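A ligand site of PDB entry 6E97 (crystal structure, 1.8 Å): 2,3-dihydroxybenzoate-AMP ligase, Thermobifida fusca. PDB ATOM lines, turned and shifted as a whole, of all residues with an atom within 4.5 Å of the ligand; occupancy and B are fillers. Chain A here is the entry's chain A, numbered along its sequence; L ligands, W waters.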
ATOM      1  N   GLY A 197      37.031  -5.525  31.757  1.00  0.00           N
ATOM      2  CA  GLY A 197      36.348  -4.254  31.635  1.00  0.00           C
ATOM      3  C   GLY A 197      36.957  -3.182  32.529  1.00  0.00           C
ATOM      4  O   GLY A 197      37.108  -2.034  32.110  1.00  0.00           O
ATOM      5  N   HIS A 240      37.826  -8.329  20.808  1.00  0.00           N
ATOM      6  CA  HIS A 240      37.044  -8.355  22.031  1.00  0.00           C
ATOM      7  C   HIS A 240      36.435  -9.748  22.219  1.00  0.00           C
ATOM      8  O   HIS A 240      36.126 -10.455  21.266  1.00  0.00           O
ATOM      9  CB  HIS A 240      35.956  -7.289  22.009  1.00  0.00           C
ATOM     10  CG  HIS A 240      35.156  -7.225  23.282  1.00  0.00           C
ATOM     11  ND1 HIS A 240      34.090  -8.061  23.533  1.00  0.00           N
ATOM     12  CD2 HIS A 240      35.295  -6.447  24.375  1.00  0.00           C
ATOM     13  CE1 HIS A 240      33.596  -7.791  24.731  1.00  0.00           C
ATOM     14  NE2 HIS A 240      34.319  -6.821  25.266  1.00  0.00           N
ATOM     15  N   ASN A 241      36.276 -10.151  23.485  1.00  0.00           N
ATOM     16  CA  ASN A 241      35.821 -11.504  23.798  1.00  0.00           C
ATOM     17  C   ASN A 241      34.561 -11.881  23.014  1.00  0.00           C
ATOM     18  O   ASN A 241      34.422 -13.017  22.539  1.00  0.00           O
ATOM     19  CB  ASN A 241      35.552 -11.613  25.307  1.00  0.00           C
ATOM     20  CG  ASN A 241      35.616 -13.043  25.795  1.00  0.00           C
ATOM     21  OD1 ASN A 241      36.562 -13.763  25.512  1.00  0.00           O
ATOM     22  ND2 ASN A 241      34.597 -13.459  26.540  1.00  0.00           N
ATOM     23  N   PHE A 242      33.619 -10.939  22.894  1.00  0.00           N
ATOM     24  CA  PHE A 242      32.334 -11.213  22.250  1.00  0.00           C
ATOM     25  C   PHE A 242      32.491 -11.556  20.767  1.00  0.00           C
ATOM     26  O   PHE A 242      32.030 -12.636  20.346  1.00  0.00           O
ATOM     27  CB  PHE A 242      31.431  -9.993  22.501  1.00  0.00           C
ATOM     28  CG  PHE A 242      30.013 -10.120  22.007  1.00  0.00           C
ATOM     29  CD1 PHE A 242      29.487 -11.343  21.616  1.00  0.00           C
ATOM     30  CD2 PHE A 242      29.202  -8.999  21.946  1.00  0.00           C
ATOM     31  CE1 PHE A 242      28.172 -11.439  21.167  1.00  0.00           C
ATOM     32  CE2 PHE A 242      27.892  -9.087  21.507  1.00  0.00           C
ATOM     33  CZ  PHE A 242      27.375 -10.305  21.107  1.00  0.00           C
ATOM     34  N   SER A 246      32.222 -15.709  20.952  1.00  0.00           N
ATOM     35  CA  SER A 246      30.843 -15.912  21.406  1.00  0.00           C
ATOM     36  C   SER A 246      29.809 -15.781  20.286  1.00  0.00           C
ATOM     37  O   SER A 246      28.853 -15.000  20.399  1.00  0.00           O
ATOM     38  CB  SER A 246      30.520 -14.933  22.537  1.00  0.00           C
ATOM     39  OG  SER A 246      31.444 -15.068  23.589  1.00  0.00           O
ATOM     40  N   GLY A 315      24.714  -7.887  22.596  1.00  0.00           N
ATOM     41  CA  GLY A 315      25.278  -8.128  23.900  1.00  0.00           C
ATOM     42  C   GLY A 315      26.225  -7.020  24.310  1.00  0.00           C
ATOM     43  O   GLY A 315      26.402  -6.035  23.602  1.00  0.00           O
ATOM     44  N   GLY A 316      26.843  -7.202  25.486  1.00  0.00           N
ATOM     45  CA  GLY A 316      27.792  -6.263  26.031  1.00  0.00           C
ATOM     46  C   GLY A 316      27.180  -5.221  26.946  1.00  0.00           C
ATOM     47  O   GLY A 316      27.869  -4.675  27.813  1.00  0.00           O
ATOM     48  N   ALA A 317      25.896  -4.926  26.746  1.00  0.00           N
ATOM     49  CA  ALA A 317      25.140  -3.965  27.551  1.00  0.00           C
ATOM     50  C   ALA A 317      23.671  -4.353  27.465  1.00  0.00           C
ATOM     51  O   ALA A 317      23.272  -5.154  26.616  1.00  0.00           O
ATOM     52  CB  ALA A 317      25.365  -2.529  27.061  1.00  0.00           C
ATOM     53  N   LYS A 318      22.877  -3.768  28.353  1.00  0.00           N
ATOM     54  CA  LYS A 318      21.465  -4.120  28.447  1.00  0.00           C
ATOM     55  C   LYS A 318      20.697  -3.698  27.186  1.00  0.00           C
ATOM     56  O   LYS A 318      20.874  -2.585  26.692  1.00  0.00           O
ATOM     57  CB  LYS A 318      20.858  -3.483  29.689  1.00  0.00           C
ATOM     58  CG  LYS A 318      19.385  -3.765  29.909  1.00  0.00           C
ATOM     59  CD  LYS A 318      19.138  -5.212  30.315  1.00  0.00           C
ATOM     60  CE  LYS A 318      17.676  -5.411  30.633  1.00  0.00           C
ATOM     61  NZ  LYS A 318      17.444  -6.708  31.294  1.00  0.00           N
ATOM     62  N   VAL A 338      23.185 -12.027  24.286  1.00  0.00           N
ATOM     63  CA  VAL A 338      24.426 -12.636  24.746  1.00  0.00           C
ATOM     64  C   VAL A 338      24.932 -11.781  25.905  1.00  0.00           C
ATOM     65  O   VAL A 338      25.282 -10.610  25.721  1.00  0.00           O
ATOM     66  CB  VAL A 338      25.471 -12.722  23.628  1.00  0.00           C
ATOM     67  CG1 VAL A 338      26.665 -13.548  24.077  1.00  0.00           C
ATOM     68  CG2 VAL A 338      24.851 -13.318  22.389  1.00  0.00           C
ATOM     69  N   PHE A 339      24.968 -12.381  27.097  1.00  0.00           N
ATOM     70  CA  PHE A 339      25.449 -11.747  28.319  1.00  0.00           C
ATOM     71  C   PHE A 339      26.698 -12.537  28.713  1.00  0.00           C
ATOM     72  O   PHE A 339      26.600 -13.624  29.259  1.00  0.00           O
ATOM     73  CB  PHE A 339      24.362 -11.760  29.397  1.00  0.00           C
ATOM     74  CG  PHE A 339      24.862 -11.548  30.818  1.00  0.00           C
ATOM     75  CD1 PHE A 339      25.820 -10.590  31.109  1.00  0.00           C
ATOM     76  CD2 PHE A 339      24.325 -12.286  31.863  1.00  0.00           C
ATOM     77  CE1 PHE A 339      26.260 -10.403  32.410  1.00  0.00           C
ATOM     78  CE2 PHE A 339      24.765 -12.098  33.164  1.00  0.00           C
ATOM     79  CZ  PHE A 339      25.733 -11.150  33.437  1.00  0.00           C
ATOM     80  N   GLY A 340      27.875 -11.975  28.431  1.00  0.00           N
ATOM     81  CA  GLY A 340      29.122 -12.659  28.705  1.00  0.00           C
ATOM     82  C   GLY A 340      30.112 -11.736  29.381  1.00  0.00           C
ATOM     83  O   GLY A 340      29.827 -10.567  29.659  1.00  0.00           O
ATOM     84  N   MET A 341      31.298 -12.275  29.644  1.00  0.00           N
ATOM     85  CA  MET A 341      32.346 -11.468  30.236  1.00  0.00           C
ATOM     86  C   MET A 341      33.694 -12.060  29.879  1.00  0.00           C
ATOM     87  O   MET A 341      33.834 -13.274  29.712  1.00  0.00           O
ATOM     88  CB  MET A 341      32.167 -11.363  31.754  1.00  0.00           C
ATOM     89  CG  MET A 341      32.066 -12.719  32.432  1.00  0.00           C
ATOM     90  SD  MET A 341      31.185 -12.644  34.006  1.00  0.00           S
ATOM     91  CE  MET A 341      29.497 -12.587  33.401  1.00  0.00           C
ATOM     92  N   ALA A 342      34.702 -11.189  29.769  1.00  0.00           N
ATOM     93  CA  ALA A 342      36.057 -11.623  29.431  1.00  0.00           C
ATOM     94  C   ALA A 342      36.622 -12.592  30.466  1.00  0.00           C
ATOM     95  O   ALA A 342      37.516 -13.383  30.130  1.00  0.00           O
ATOM     96  CB  ALA A 342      36.971 -10.414  29.278  1.00  0.00           C
ATOM     97  N   GLU A 343      36.115 -12.553  31.700  1.00  0.00           N
ATOM     98  CA  GLU A 343      36.603 -13.436  32.756  1.00  0.00           C
ATOM     99  C   GLU A 343      36.087 -14.864  32.607  1.00  0.00           C
ATOM    100  O   GLU A 343      36.624 -15.772  33.246  1.00  0.00           O
ATOM    101  CB  GLU A 343      36.190 -12.883  34.128  1.00  0.00           C
ATOM    102  CG  GLU A 343      36.978 -11.665  34.625  1.00  0.00           C
ATOM    103  CD  GLU A 343      36.420 -10.328  34.132  1.00  0.00           C
ATOM    104  OE1 GLU A 343      35.439 -10.327  33.366  1.00  0.00           O
ATOM    105  OE2 GLU A 343      36.981  -9.293  34.503  1.00  0.00           O
ATOM    106  N   VAL A 346      29.561 -17.000  29.757  1.00  0.00           N
ATOM    107  CA  VAL A 346      28.789 -16.484  28.630  1.00  0.00           C
ATOM    108  C   VAL A 346      27.416 -17.142  28.643  1.00  0.00           C
ATOM    109  O   VAL A 346      27.302 -18.361  28.779  1.00  0.00           O
ATOM    110  CB  VAL A 346      29.484 -16.737  27.272  1.00  0.00           C
ATOM    111  CG1 VAL A 346      28.635 -16.179  26.150  1.00  0.00           C
ATOM    112  CG2 VAL A 346      30.867 -16.136  27.266  1.00  0.00           C
ATOM    113  N   GLN A 362      18.509 -12.348  29.023  1.00  0.00           N
ATOM    114  CA  GLN A 362      19.859 -12.333  28.498  1.00  0.00           C
ATOM    115  C   GLN A 362      20.477 -13.733  28.416  1.00  0.00           C
ATOM    116  O   GLN A 362      21.707 -13.862  28.369  1.00  0.00           O
ATOM    117  CB  GLN A 362      20.742 -11.398  29.337  1.00  0.00           C
ATOM    118  CG  GLN A 362      20.556  -9.912  29.038  1.00  0.00           C
ATOM    119  CD  GLN A 362      19.210  -9.364  29.490  1.00  0.00           C
ATOM    120  OE1 GLN A 362      18.936  -9.295  30.679  1.00  0.00           O
ATOM    121  NE2 GLN A 362      18.371  -8.973  28.545  1.00  0.00           N
ATOM    122  N   THR A 420      31.087 -11.377  39.700  1.00  0.00           N
ATOM    123  CA  THR A 420      30.928 -10.674  38.428  1.00  0.00           C
ATOM    124  C   THR A 420      30.677  -9.186  38.626  1.00  0.00           C
ATOM    125  O   THR A 420      31.002  -8.379  37.744  1.00  0.00           O
ATOM    126  CB  THR A 420      29.791 -11.263  37.600  1.00  0.00           C
ATOM    127  OG1 THR A 420      28.542 -10.966  38.230  1.00  0.00           O
ATOM    128  CG2 THR A 420      29.928 -12.776  37.425  1.00  0.00           C
ATOM    129  N   ASP A 422      27.635  -8.064  38.778  1.00  0.00           N
ATOM    130  CA  ASP A 422      26.350  -7.855  38.137  1.00  0.00           C
ATOM    131  C   ASP A 422      25.214  -8.193  39.090  1.00  0.00           C
ATOM    132  O   ASP A 422      25.347  -9.077  39.954  1.00  0.00           O
ATOM    133  CB  ASP A 422      26.239  -8.705  36.862  1.00  0.00           C
ATOM    134  CG  ASP A 422      27.195  -8.241  35.788  1.00  0.00           C
ATOM    135  OD1 ASP A 422      27.242  -7.024  35.538  1.00  0.00           O
ATOM    136  OD2 ASP A 422      27.914  -9.097  35.233  1.00  0.00           O
ATOM    137  N   VAL A 434      19.535  -9.374  33.411  1.00  0.00           N
ATOM    138  CA  VAL A 434      20.464  -8.417  33.992  1.00  0.00           C
ATOM    139  C   VAL A 434      19.676  -7.181  34.414  1.00  0.00           C
ATOM    140  O   VAL A 434      19.049  -6.513  33.585  1.00  0.00           O
ATOM    141  CB  VAL A 434      21.585  -8.059  33.004  1.00  0.00           C
ATOM    142  CG1 VAL A 434      22.555  -7.080  33.652  1.00  0.00           C
ATOM    143  CG2 VAL A 434      22.326  -9.315  32.556  1.00  0.00           C
ATOM    144  N   LYS A 439      29.416  -3.215  40.737  1.00  0.00           N
ATOM    145  CA  LYS A 439      30.784  -2.734  40.605  1.00  0.00           C
ATOM    146  C   LYS A 439      30.828  -1.291  40.125  1.00  0.00           C
ATOM    147  O   LYS A 439      29.920  -0.822  39.436  1.00  0.00           O
ATOM    148  CB  LYS A 439      31.547  -3.622  39.623  1.00  0.00           C
ATOM    149  CG  LYS A 439      30.839  -3.805  38.297  1.00  0.00           C
ATOM    150  CD  LYS A 439      31.478  -4.907  37.494  1.00  0.00           C
ATOM    151  CE  LYS A 439      30.529  -5.376  36.414  1.00  0.00           C
ATOM    152  NZ  LYS A 439      31.111  -6.564  35.740  1.00  0.00           N
ATOM    153  N   GLN A 441      31.557   0.773  37.626  1.00  0.00           N
ATOM    154  CA  GLN A 441      31.845   0.639  36.210  1.00  0.00           C
ATOM    155  C   GLN A 441      30.711   1.156  35.348  1.00  0.00           C
ATOM    156  O   GLN A 441      29.644   0.540  35.266  1.00  0.00           O
ATOM    157  CB  GLN A 441      32.116  -0.825  35.861  1.00  0.00           C
ATOM    158  CG  GLN A 441      32.479  -1.039  34.403  1.00  0.00           C
ATOM    159  CD  GLN A 441      32.571  -2.497  34.054  1.00  0.00           C
ATOM    160  OE1 GLN A 441      31.566  -3.145  33.771  1.00  0.00           O
ATOM    161  NE2 GLN A 441      33.778  -3.032  34.075  1.00  0.00           N
ATOM    162  N   ASN A 443      28.825   1.576  32.037  1.00  0.00           N
ATOM    163  CA  ASN A 443      28.724   0.800  30.808  1.00  0.00           C
ATOM    164  C   ASN A 443      28.179   1.708  29.720  1.00  0.00           C
ATOM    165  O   ASN A 443      26.962   1.859  29.574  1.00  0.00           O
ATOM    166  CB  ASN A 443      27.858  -0.438  31.002  1.00  0.00           C
ATOM    167  CG  ASN A 443      27.953  -1.381  29.830  1.00  0.00           C
ATOM    168  OD1 ASN A 443      28.443  -0.996  28.764  1.00  0.00           O
ATOM    169  ND2 ASN A 443      27.493  -2.607  30.010  1.00  0.00           N
ATOM    170  N   LYS A 448      33.379  -0.261  28.718  1.00  0.00           N
ATOM    171  CA  LYS A 448      33.371  -0.144  30.172  1.00  0.00           C
ATOM    172  C   LYS A 448      34.352   0.935  30.620  1.00  0.00           C
ATOM    173  O   LYS A 448      35.498   0.978  30.170  1.00  0.00           O
ATOM    174  CB  LYS A 448      33.719  -1.477  30.832  1.00  0.00           C
ATOM    175  CG  LYS A 448      33.068  -2.694  30.176  1.00  0.00           C
ATOM    176  CD  LYS A 448      31.554  -2.598  30.147  1.00  0.00           C
ATOM    177  CE  LYS A 448      30.901  -3.938  29.784  1.00  0.00           C
ATOM    178  NZ  LYS A 448      31.138  -4.395  28.385  1.00  0.00           N
HETATM  179  C1  LIG L   1      23.773  -6.481  30.251  1.00  0.00           C
HETATM  180  N1  LIG L   1      25.074  -6.385  30.576  1.00  0.00           N
HETATM  181  C2  LIG L   1      26.013  -7.081  29.893  1.00  0.00           C
HETATM  182  C3  LIG L   1      24.154  -8.016  28.502  1.00  0.00           C
HETATM  183  C4  LIG L   1      27.773  -8.035  29.024  1.00  0.00           C
HETATM  184  C5  LIG L   1      29.717 -12.179  25.086  1.00  0.00           C
HETATM  185  C6  LIG L   1      28.900 -11.067  25.300  1.00  0.00           C
HETATM  186  C7  LIG L   1      29.365  -9.928  25.971  1.00  0.00           C
HETATM  187  C8  LIG L   1      30.672  -9.857  26.461  1.00  0.00           C
HETATM  188  C9  LIG L   1      31.182  -8.640  27.186  1.00  0.00           C
HETATM  189  C10 LIG L   1      31.568 -11.016  26.265  1.00  0.00           C
HETATM  190  C11 LIG L   1      25.602  -7.961  28.794  1.00  0.00           C
HETATM  191  N2  LIG L   1      23.320  -7.265  29.269  1.00  0.00           N
HETATM  192  N3  LIG L   1      23.680  -8.791  27.516  1.00  0.00           N
HETATM  193  O1  LIG L   1      32.835 -10.972  26.730  1.00  0.00           O
HETATM  194  O2  LIG L   1      31.827 -13.292  25.326  1.00  0.00           O
HETATM  195  C12 LIG L   1      28.164  -6.440  30.940  1.00  0.00           C
HETATM  196  C13 LIG L   1      28.127  -7.042  32.343  1.00  0.00           C
HETATM  197  C14 LIG L   1      29.333  -7.973  32.273  1.00  0.00           C
HETATM  198  C15 LIG L   1      30.338  -7.116  31.512  1.00  0.00           C
HETATM  199  C16 LIG L   1      31.493  -7.834  30.858  1.00  0.00           C
HETATM  200  C17 LIG L   1      31.030 -12.203  25.544  1.00  0.00           C
HETATM  201  N4  LIG L   1      26.724  -8.523  28.305  1.00  0.00           N
HETATM  202  N5  LIG L   1      27.337  -7.181  29.972  1.00  0.00           N
HETATM  203  O3  LIG L   1      30.506  -7.627  27.135  1.00  0.00           O
HETATM  204  O4  LIG L   1      34.339  -8.017  29.726  1.00  0.00           O
HETATM  205  O5  LIG L   1      28.353  -5.977  33.244  1.00  0.00           O
HETATM  206  O6  LIG L   1      32.452  -8.706  27.924  1.00  0.00           O
HETATM  207  O7  LIG L   1      29.806  -8.424  33.527  1.00  0.00           O
HETATM  208  O8  LIG L   1      33.464  -6.415  27.928  1.00  0.00           O
HETATM  209  O9  LIG L   1      29.511  -6.460  30.508  1.00  0.00           O
HETATM  210  O10 LIG L   1      32.153  -6.991  29.927  1.00  0.00           O
HETATM  211  P1  LIG L   1      33.180  -7.577  28.855  1.00  0.00           P
HETATM  212  O   HOH W   1      25.463  -5.422  35.012  1.00  0.00           O
HETATM  213  O   HOH W   2      28.549  -3.197  32.950  1.00  0.00           O
HETATM  214  O   HOH W   3      25.262  -4.021  32.285  1.00  0.00           O
HETATM  215  O   HOH W   4      35.305  -7.762  32.117  1.00  0.00           O
HETATM  216  O   HOH W   5      32.623  -9.393  34.923  1.00  0.00           O
HETATM  217  O   HOH W   6      21.363  -8.392  25.354  1.00  0.00           O
HETATM  218  O   HOH W   7      35.416  -4.684  27.910  1.00  0.00           O
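An oxygen (O2) of the ligand sits at hydrogen-bond distance from the side-chain hydroxyl (OG) of Ser 246 (2.5 Å).
An oxygen (O7) of the ligand sits at hydrogen-bond distance from the side-chain carboxylate of Asp 422 (2.6 Å).
NE2 of His 240 lies within hydrogen-bond range of O8 of the ligand.
The side-chain amino group (NZ) of Lys 448 is in salt-bridge range of an oxygen (O8) of the ligand, at 3.1 Å.
O of Val 338 is in hydrogen-bond range of N3 of the ligand, at 3.0 Å.
The side-chain amide nitrogen (ND2) of Asn 241 is in hydrogen-bond range of an oxygen (O2) of the ligand, at 3.0 Å.
N of Gly 316 sits at hydrogen-bond distance from N4 of the ligand, 3.1 Å away.
O7 of the ligand is in hydrogen-bond range of NZ of Lys 439.
An oxygen (O4) of the ligand sits at hydrogen-bond distance from the backbone NH of Ala 342.
OD1 of Asp 422 is in salt-bridge range of NZ of Lys 439 (3.9 Å).
ND1 of His 240 lies within hydrogen-bond range of N of Phe 242.
NZ of Lys 448 sits at hydrogen-bond distance from O of Gly 316, 3.3 Å away.
The backbone carbonyl oxygen (O) of Met 341 lies within hydrogen-bond range of the side-chain amide nitrogen (ND2) of Asn 241 (3.3 Å).
NZ of Lys 439 lies within hydrogen-bond range of O of Thr 420, 2.7 Å away.
The side-chain amino group (NZ) of Lys 318 is in hydrogen-bond range of the side-chain amide oxygen (OE1) of Gln 362.
The backbone carbonyl oxygen (O) of Val 434 sits at hydrogen-bond distance from the side-chain amino group (NZ) of Lys 318, 2.8 Å away.
OE1 of Gln 362 lies within hydrogen-bond range of N of Val 434 (2.8 Å).
N2 of the ligand sits close to O of Ala 317, 3.4 Å away.
CD1 of Phe 242 touches C5 of the ligand, 3.6 Å away.
Lys 318 touches the ligand (N to C1, 3.4 Å).
CA of Phe 339 touches N4 of the ligand, at 3.5 Å.
Gly 340 touches the ligand.
Met 341 touches the ligand.
CG2 of Val 346 touches O2 of the ligand, 3.6 Å away.
Gln 362 touches the ligand (CG to N3, 3.7 Å).
Val 434 touches the ligand (CG1 to C1, 3.7 Å).
Hydrophobic or aromatic side chains that line the ligand: His 240, Phe 242, Val 338, Phe 339, Met 341, Ala 342, Val 346 and Val 434.
The nearest printed residue that does not touch the ligand is Asn 443 (4.001 Å).
Water W4 lies within hydrogen-bond range of O4 of the ligand (2.6 Å), N of Gly 197 (2.8 Å) and OE1 of Glu 343 (2.9 Å).
Water W2 lies within hydrogen-bond range of an oxygen (O5) of the ligand (2.8 Å), the side-chain amide oxygen (OE1) of Gln 441 (3.1 Å) and the side-chain amide nitrogen (ND2) of Asn 443 (3.2 Å).
Water W3 bridges N1 of the ligand (2.9 Å) and ND2 of Asn 443 (3.5 Å).
Water W1 lies within hydrogen-bond range of OD1 of Asp 422 and O5 of the ligand.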
